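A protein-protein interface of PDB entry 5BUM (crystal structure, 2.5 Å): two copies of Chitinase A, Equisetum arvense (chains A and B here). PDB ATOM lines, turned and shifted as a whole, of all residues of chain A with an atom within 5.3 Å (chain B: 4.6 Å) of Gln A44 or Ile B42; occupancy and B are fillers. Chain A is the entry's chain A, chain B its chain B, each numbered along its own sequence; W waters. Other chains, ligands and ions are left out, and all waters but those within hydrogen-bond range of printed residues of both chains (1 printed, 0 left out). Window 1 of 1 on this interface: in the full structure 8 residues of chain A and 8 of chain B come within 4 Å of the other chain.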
ATOM      1  N   TYR A   6      16.406 -30.497  -5.586  1.00  0.00           N
ATOM      2  CA  TYR A   6      17.732 -31.038  -5.765  1.00  0.00           C
ATOM      3  C   TYR A   6      18.791 -30.108  -5.170  1.00  0.00           C
ATOM      4  O   TYR A   6      18.783 -28.904  -5.412  1.00  0.00           O
ATOM      5  CB  TYR A   6      18.063 -31.235  -7.266  1.00  0.00           C
ATOM      6  CG  TYR A   6      19.464 -31.787  -7.447  1.00  0.00           C
ATOM      7  CD1 TYR A   6      19.740 -33.110  -7.176  1.00  0.00           C
ATOM      8  CD2 TYR A   6      20.494 -30.975  -7.816  1.00  0.00           C
ATOM      9  CE1 TYR A   6      21.023 -33.630  -7.321  1.00  0.00           C
ATOM     10  CE2 TYR A   6      21.782 -31.454  -7.959  1.00  0.00           C
ATOM     11  CZ  TYR A   6      22.047 -32.786  -7.730  1.00  0.00           C
ATOM     12  OH  TYR A   6      23.352 -33.266  -7.855  1.00  0.00           O
ATOM     13  N   THR A   7      19.741 -30.682  -4.449  1.00  0.00           N
ATOM     14  CA  THR A   7      20.773 -29.930  -3.778  1.00  0.00           C
ATOM     15  C   THR A   7      22.070 -29.901  -4.543  1.00  0.00           C
ATOM     16  O   THR A   7      22.723 -30.927  -4.719  1.00  0.00           O
ATOM     17  CB  THR A   7      21.102 -30.590  -2.436  1.00  0.00           C
ATOM     18  OG1 THR A   7      19.962 -30.471  -1.570  1.00  0.00           O
ATOM     19  CG2 THR A   7      22.353 -29.901  -1.803  1.00  0.00           C
ATOM     20  N   VAL A   8      22.514 -28.722  -4.942  1.00  0.00           N
ATOM     21  CA  VAL A   8      23.745 -28.643  -5.724  1.00  0.00           C
ATOM     22  C   VAL A   8      24.921 -29.244  -4.933  1.00  0.00           C
ATOM     23  O   VAL A   8      25.051 -29.052  -3.714  1.00  0.00           O
ATOM     24  CB  VAL A   8      24.015 -27.206  -6.171  1.00  0.00           C
ATOM     25  CG1 VAL A   8      25.379 -27.089  -6.815  1.00  0.00           C
ATOM     26  CG2 VAL A   8      22.921 -26.736  -7.107  1.00  0.00           C
ATOM     27  N   ASN A  32      12.796 -22.014 -11.212  1.00  0.00           N
ATOM     28  CA  ASN A  32      13.666 -21.326 -10.267  1.00  0.00           C
ATOM     29  C   ASN A  32      13.895 -19.869 -10.729  1.00  0.00           C
ATOM     30  O   ASN A  32      14.933 -19.564 -11.347  1.00  0.00           O
ATOM     31  CB  ASN A  32      15.011 -22.081 -10.114  1.00  0.00           C
ATOM     32  CG  ASN A  32      14.846 -23.478  -9.541  1.00  0.00           C
ATOM     33  OD1 ASN A  32      14.843 -23.645  -8.320  1.00  0.00           O
ATOM     34  ND2 ASN A  32      14.726 -24.504 -10.420  1.00  0.00           N
ATOM     35  N   PRO A  33      12.931 -18.969 -10.421  1.00  0.00           N
ATOM     36  CA  PRO A  33      13.034 -17.560 -10.845  1.00  0.00           C
ATOM     37  C   PRO A  33      14.416 -16.923 -10.571  1.00  0.00           C
ATOM     38  O   PRO A  33      14.859 -16.828  -9.421  1.00  0.00           O
ATOM     39  CB  PRO A  33      11.932 -16.879 -10.009  1.00  0.00           C
ATOM     40  CG  PRO A  33      10.878 -17.940  -9.854  1.00  0.00           C
ATOM     41  CD  PRO A  33      11.678 -19.220  -9.661  1.00  0.00           C
ATOM     42  N   GLY A  34      15.106 -16.530 -11.630  1.00  0.00           N
ATOM     43  CA  GLY A  34      16.399 -15.874 -11.501  1.00  0.00           C
ATOM     44  C   GLY A  34      17.592 -16.803 -11.366  1.00  0.00           C
ATOM     45  O   GLY A  34      18.700 -16.326 -11.100  1.00  0.00           O
ATOM     46  N   LEU A  35      17.397 -18.118 -11.544  1.00  0.00           N
ATOM     47  CA  LEU A  35      18.536 -19.085 -11.553  1.00  0.00           C
ATOM     48  C   LEU A  35      19.683 -18.577 -12.398  1.00  0.00           C
ATOM     49  O   LEU A  35      19.447 -17.965 -13.430  1.00  0.00           O
ATOM     50  CB  LEU A  35      18.078 -20.451 -12.074  1.00  0.00           C
ATOM     51  CG  LEU A  35      19.123 -21.555 -12.168  1.00  0.00           C
ATOM     52  CD1 LEU A  35      19.823 -21.744 -10.835  1.00  0.00           C
ATOM     53  CD2 LEU A  35      18.510 -22.869 -12.621  1.00  0.00           C
ATOM     54  N   ASN A  39      26.744 -19.970 -12.109  1.00  0.00           N
ATOM     55  CA  ASN A  39      27.035 -19.469 -10.784  1.00  0.00           C
ATOM     56  C   ASN A  39      26.240 -20.198  -9.708  1.00  0.00           C
ATOM     57  O   ASN A  39      25.606 -19.581  -8.842  1.00  0.00           O
ATOM     58  CB  ASN A  39      26.678 -17.982 -10.754  1.00  0.00           C
ATOM     59  CG  ASN A  39      27.115 -17.297  -9.469  1.00  0.00           C
ATOM     60  OD1 ASN A  39      26.454 -16.353  -9.026  1.00  0.00           O
ATOM     61  ND2 ASN A  39      28.223 -17.761  -8.867  1.00  0.00           N
ATOM     62  N   LEU A  40      26.254 -21.518  -9.795  1.00  0.00           N
ATOM     63  CA  LEU A  40      25.563 -22.324  -8.835  1.00  0.00           C
ATOM     64  C   LEU A  40      26.436 -22.417  -7.606  1.00  0.00           C
ATOM     65  O   LEU A  40      27.666 -22.506  -7.711  1.00  0.00           O
ATOM     66  CB  LEU A  40      25.370 -23.718  -9.385  1.00  0.00           C
ATOM     67  CG  LEU A  40      24.483 -23.859 -10.592  1.00  0.00           C
ATOM     68  CD1 LEU A  40      24.512 -25.286 -11.095  1.00  0.00           C
ATOM     69  CD2 LEU A  40      23.085 -23.457 -10.207  1.00  0.00           C
ATOM     70  N   GLN A  41      25.787 -22.435  -6.449  1.00  0.00           N
ATOM     71  CA  GLN A  41      26.463 -22.546  -5.138  1.00  0.00           C
ATOM     72  C   GLN A  41      26.277 -23.950  -4.533  1.00  0.00           C
ATOM     73  O   GLN A  41      25.184 -24.554  -4.627  1.00  0.00           O
ATOM     74  CB  GLN A  41      25.816 -21.543  -4.170  1.00  0.00           C
ATOM     75  CG  GLN A  41      25.505 -20.162  -4.752  1.00  0.00           C
ATOM     76  CD  GLN A  41      26.761 -19.448  -5.158  1.00  0.00           C
ATOM     77  OE1 GLN A  41      26.846 -18.881  -6.238  1.00  0.00           O
ATOM     78  NE2 GLN A  41      27.762 -19.510  -4.312  1.00  0.00           N
ATOM     79  N   ILE A  42      27.302 -24.454  -3.874  1.00  0.00           N
ATOM     80  CA  ILE A  42      27.171 -25.711  -3.154  1.00  0.00           C
ATOM     81  C   ILE A  42      26.015 -25.637  -2.144  1.00  0.00           C
ATOM     82  O   ILE A  42      25.858 -24.640  -1.448  1.00  0.00           O
ATOM     83  CB  ILE A  42      28.505 -26.087  -2.487  1.00  0.00           C
ATOM     84  CG1 ILE A  42      29.440 -26.727  -3.530  1.00  0.00           C
ATOM     85  CG2 ILE A  42      28.301 -27.085  -1.373  1.00  0.00           C
ATOM     86  CD1 ILE A  42      30.887 -26.343  -3.348  1.00  0.00           C
ATOM     87  N   GLY A  43      25.174 -26.673  -2.092  1.00  0.00           N
ATOM     88  CA  GLY A  43      24.038 -26.691  -1.177  1.00  0.00           C
ATOM     89  C   GLY A  43      22.843 -25.896  -1.664  1.00  0.00           C
ATOM     90  O   GLY A  43      21.750 -25.912  -1.056  1.00  0.00           O
ATOM     91  N   GLN A  44      23.009 -25.177  -2.756  1.00  0.00           N
ATOM     92  CA  GLN A  44      21.877 -24.396  -3.308  1.00  0.00           C
ATOM     93  C   GLN A  44      20.756 -25.379  -3.621  1.00  0.00           C
ATOM     94  O   GLN A  44      21.002 -26.431  -4.159  1.00  0.00           O
ATOM     95  CB  GLN A  44      22.362 -23.685  -4.564  1.00  0.00           C
ATOM     96  CG  GLN A  44      21.360 -22.774  -5.295  1.00  0.00           C
ATOM     97  CD  GLN A  44      22.005 -22.110  -6.509  1.00  0.00           C
ATOM     98  OE1 GLN A  44      23.184 -22.361  -6.799  1.00  0.00           O
ATOM     99  NE2 GLN A  44      21.243 -21.285  -7.229  1.00  0.00           N
ATOM    100  N   GLN A  45      19.532 -25.066  -3.276  1.00  0.00           N
ATOM    101  CA  GLN A  45      18.424 -25.997  -3.461  1.00  0.00           C
ATOM    102  C   GLN A  45      17.651 -25.543  -4.617  1.00  0.00           C
ATOM    103  O   GLN A  45      17.299 -24.378  -4.695  1.00  0.00           O
ATOM    104  CB  GLN A  45      17.506 -25.991  -2.245  1.00  0.00           C
ATOM    105  CG  GLN A  45      18.275 -26.449  -1.006  1.00  0.00           C
ATOM    106  CD  GLN A  45      17.434 -26.484   0.222  1.00  0.00           C
ATOM    107  OE1 GLN A  45      16.232 -26.179   0.185  1.00  0.00           O
ATOM    108  NE2 GLN A  45      18.064 -26.848   1.338  1.00  0.00           N
ATOM    109  N   LEU A  46      17.382 -26.463  -5.532  1.00  0.00           N
ATOM    110  CA  LEU A  46      16.796 -26.104  -6.784  1.00  0.00           C
ATOM    111  C   LEU A  46      15.504 -26.869  -6.888  1.00  0.00           C
ATOM    112  O   LEU A  46      15.481 -28.079  -6.699  1.00  0.00           O
ATOM    113  CB  LEU A  46      17.738 -26.498  -7.900  1.00  0.00           C
ATOM    114  CG  LEU A  46      18.644 -25.488  -8.617  1.00  0.00           C
ATOM    115  CD1 LEU A  46      18.947 -24.192  -7.868  1.00  0.00           C
ATOM    116  CD2 LEU A  46      19.916 -26.202  -9.029  1.00  0.00           C
ATOM    117  N   VAL B   8      17.266 -18.929   0.493  1.00  0.00           N
ATOM    118  CA  VAL B   8      16.786 -17.786  -0.286  1.00  0.00           C
ATOM    119  C   VAL B   8      15.648 -18.230  -1.196  1.00  0.00           C
ATOM    120  O   VAL B   8      15.743 -19.294  -1.812  1.00  0.00           O
ATOM    121  CB  VAL B   8      17.928 -17.208  -1.158  1.00  0.00           C
ATOM    122  CG1 VAL B   8      17.437 -16.061  -2.032  1.00  0.00           C
ATOM    123  CG2 VAL B   8      19.131 -16.818  -0.315  1.00  0.00           C
ATOM    124  N   LYS B   9      14.580 -17.436  -1.243  1.00  0.00           N
ATOM    125  CA  LYS B   9      13.421 -17.620  -2.107  1.00  0.00           C
ATOM    126  C   LYS B   9      13.379 -16.458  -3.132  1.00  0.00           C
ATOM    127  O   LYS B   9      14.175 -15.532  -3.016  1.00  0.00           O
ATOM    128  CB  LYS B   9      12.151 -17.576  -1.256  1.00  0.00           C
ATOM    129  CG  LYS B   9      12.032 -18.618  -0.138  1.00  0.00           C
ATOM    130  CD  LYS B   9      11.037 -18.133   0.925  1.00  0.00           C
ATOM    131  CE  LYS B   9      10.417 -19.242   1.772  1.00  0.00           C
ATOM    132  NZ  LYS B   9       9.046 -19.580   1.283  1.00  0.00           N
ATOM    133  N   SER B  10      12.463 -16.497  -4.113  1.00  0.00           N
ATOM    134  CA  SER B  10      12.295 -15.412  -5.110  1.00  0.00           C
ATOM    135  C   SER B  10      12.203 -14.024  -4.453  1.00  0.00           C
ATOM    136  O   SER B  10      11.306 -13.794  -3.640  1.00  0.00           O
ATOM    137  CB  SER B  10      11.002 -15.602  -5.916  1.00  0.00           C
ATOM    138  OG  SER B  10      10.967 -16.820  -6.612  1.00  0.00           O
ATOM    139  N   LEU B  40      21.753 -12.572  -5.025  1.00  0.00           N
ATOM    140  CA  LEU B  40      21.532 -13.681  -4.119  1.00  0.00           C
ATOM    141  C   LEU B  40      21.041 -14.806  -4.995  1.00  0.00           C
ATOM    142  O   LEU B  40      20.114 -14.628  -5.793  1.00  0.00           O
ATOM    143  CB  LEU B  40      20.503 -13.317  -3.034  1.00  0.00           C
ATOM    144  CG  LEU B  40      21.014 -12.426  -1.875  1.00  0.00           C
ATOM    145  CD1 LEU B  40      19.823 -11.944  -1.074  1.00  0.00           C
ATOM    146  CD2 LEU B  40      22.063 -13.081  -0.978  1.00  0.00           C
ATOM    147  N   GLN B  41      21.667 -15.959  -4.871  1.00  0.00           N
ATOM    148  CA  GLN B  41      21.214 -17.081  -5.666  1.00  0.00           C
ATOM    149  C   GLN B  41      19.935 -17.668  -5.071  1.00  0.00           C
ATOM    150  O   GLN B  41      19.830 -17.900  -3.860  1.00  0.00           O
ATOM    151  CB  GLN B  41      22.332 -18.129  -5.801  1.00  0.00           C
ATOM    152  CG  GLN B  41      23.547 -17.677  -6.631  1.00  0.00           C
ATOM    153  CD  GLN B  41      23.157 -16.855  -7.862  1.00  0.00           C
ATOM    154  OE1 GLN B  41      22.235 -17.207  -8.634  1.00  0.00           O
ATOM    155  NE2 GLN B  41      23.822 -15.717  -8.012  1.00  0.00           N
ATOM    156  N   ILE B  42      18.948 -17.879  -5.927  1.00  0.00           N
ATOM    157  CA  ILE B  42      17.776 -18.617  -5.525  1.00  0.00           C
ATOM    158  C   ILE B  42      18.147 -20.017  -4.984  1.00  0.00           C
ATOM    159  O   ILE B  42      18.899 -20.772  -5.638  1.00  0.00           O
ATOM    160  CB  ILE B  42      16.763 -18.763  -6.653  1.00  0.00           C
ATOM    161  CG1 ILE B  42      15.557 -19.522  -6.106  1.00  0.00           C
ATOM    162  CG2 ILE B  42      17.374 -19.473  -7.869  1.00  0.00           C
ATOM    163  CD1 ILE B  42      14.264 -19.100  -6.751  1.00  0.00           C
ATOM    164  N   GLY B  43      17.637 -20.314  -3.778  1.00  0.00           N
ATOM    165  CA  GLY B  43      17.958 -21.530  -3.021  1.00  0.00           C
ATOM    166  C   GLY B  43      19.281 -21.549  -2.277  1.00  0.00           C
ATOM    167  O   GLY B  43      19.629 -22.563  -1.665  1.00  0.00           O
ATOM    168  N   GLN B  44      20.036 -20.460  -2.340  1.00  0.00           N
ATOM    169  CA  GLN B  44      21.306 -20.335  -1.599  1.00  0.00           C
ATOM    170  C   GLN B  44      21.069 -20.507  -0.102  1.00  0.00           C
ATOM    171  O   GLN B  44      20.044 -20.075   0.464  1.00  0.00           O
ATOM    172  CB  GLN B  44      21.942 -18.935  -1.850  1.00  0.00           C
ATOM    173  CG  GLN B  44      23.400 -18.825  -1.384  1.00  0.00           C
ATOM    174  CD  GLN B  44      24.071 -17.489  -1.730  1.00  0.00           C
ATOM    175  OE1 GLN B  44      23.548 -16.669  -2.504  1.00  0.00           O
ATOM    176  NE2 GLN B  44      25.247 -17.269  -1.142  1.00  0.00           N
HETATM  177  O   HOH W   1      22.011 -19.629  -9.538  1.00  0.00           O
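The side-chain amide nitrogen of Gln B41 sits at hydrogen-bond distance from the side-chain amide oxygen of Asn A39, 2.9 Å away.
The backbone carbonyl oxygen (O) of Ile B42 lies within hydrogen-bond range of the side-chain amide nitrogen (NE2) of Gln A44.
O of Gly B43 is in hydrogen-bond range of N of Gln A45, at 3.0 Å.
The backbone NH (N) of Val A8 is in hydrogen-bond range of the backbone carbonyl oxygen (O) of Gln A44 (2.9 Å).
The backbone carbonyl oxygen (O) of Asn A39 lies close to the side-chain amide oxygen (OE1) of Gln A41 (3.0 Å).
The side-chain amide oxygen (OE1) of Gln A44 lies within hydrogen-bond range of the backbone NH (N) of Gln A41 (2.6 Å).
The backbone carbonyl oxygen (O) of Val B8 lies within hydrogen-bond range of the backbone NH (N) of Gly B43, 2.9 Å away.
N of Val B8 lies within hydrogen-bond range of O of Gln B44 (3.0 Å).
The side-chain amide oxygen (OE1) of Gln B44 is in hydrogen-bond range of the backbone NH (N) of Gln B41.
CG of Pro A33 touches OG of Ser B10, at 3.4 Å.
O of Pro A33 touches CD1 of Ile B42, 3.6 Å away.
Leu A35 touches Ile B42.
Gln A41 touches Gln B41.
Gln B41 touches Gln A44.
Gln A44 touches Gly B43.
Gln A44 touches Gln B44.
Of chain B, only Gln B41 (3.6 Å), Ile B42 (2.9 Å), Gly B43 (3.3 Å) and Gln B44 (3.98 Å) come within 4 Å of Gln A44.
Ile B42 touches three residues of chain A.
Of the printed residues of chain B, Gln A45 touches Gly B43.
Printed residues of chain A within 4 Å of Gly B43: Gln A44 and Gln A45.
The nearest printed residue of chain A that does not touch Ile B42 is Gln A45 (4.1 Å).
The nearest printed residue of chain B that does not touch Leu A35 is Gln B41 (4.7 Å).
Of the 15 printed residues of chain A, 6 touch a printed residue of chain B.
Hydrophobic or aromatic side chains of chain A that line the printed part of chain B: Pro A33.
Among the printed residues, 10 pairs touch across the chains.
Among the printed residues, no Asp or Glu carboxylate lies within 4 Å of a Lys or Arg side-chain nitrogen of the other chain.
Gln A41 touches its own counterpart, Gln B41.
Gln A44 touches Ile B42, but with the chains exchanged Ile A42 does not touch Gln B44 (6.3 Å).
Gln A44 touches Gly B43, but with the chains exchanged Gly A43 does not touch Gln B44 (5.5 Å).
Gln A44 touches its own counterpart, Gln B44.
Of the 10 pairs that touch across the chains among the printed residues, 2 have their exchanged pair printed and touching as well.
Water W1 lies within hydrogen-bond range of OE1 of Gln B41 (2.6 Å) and NE2 of Gln A44 (2.9 Å).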
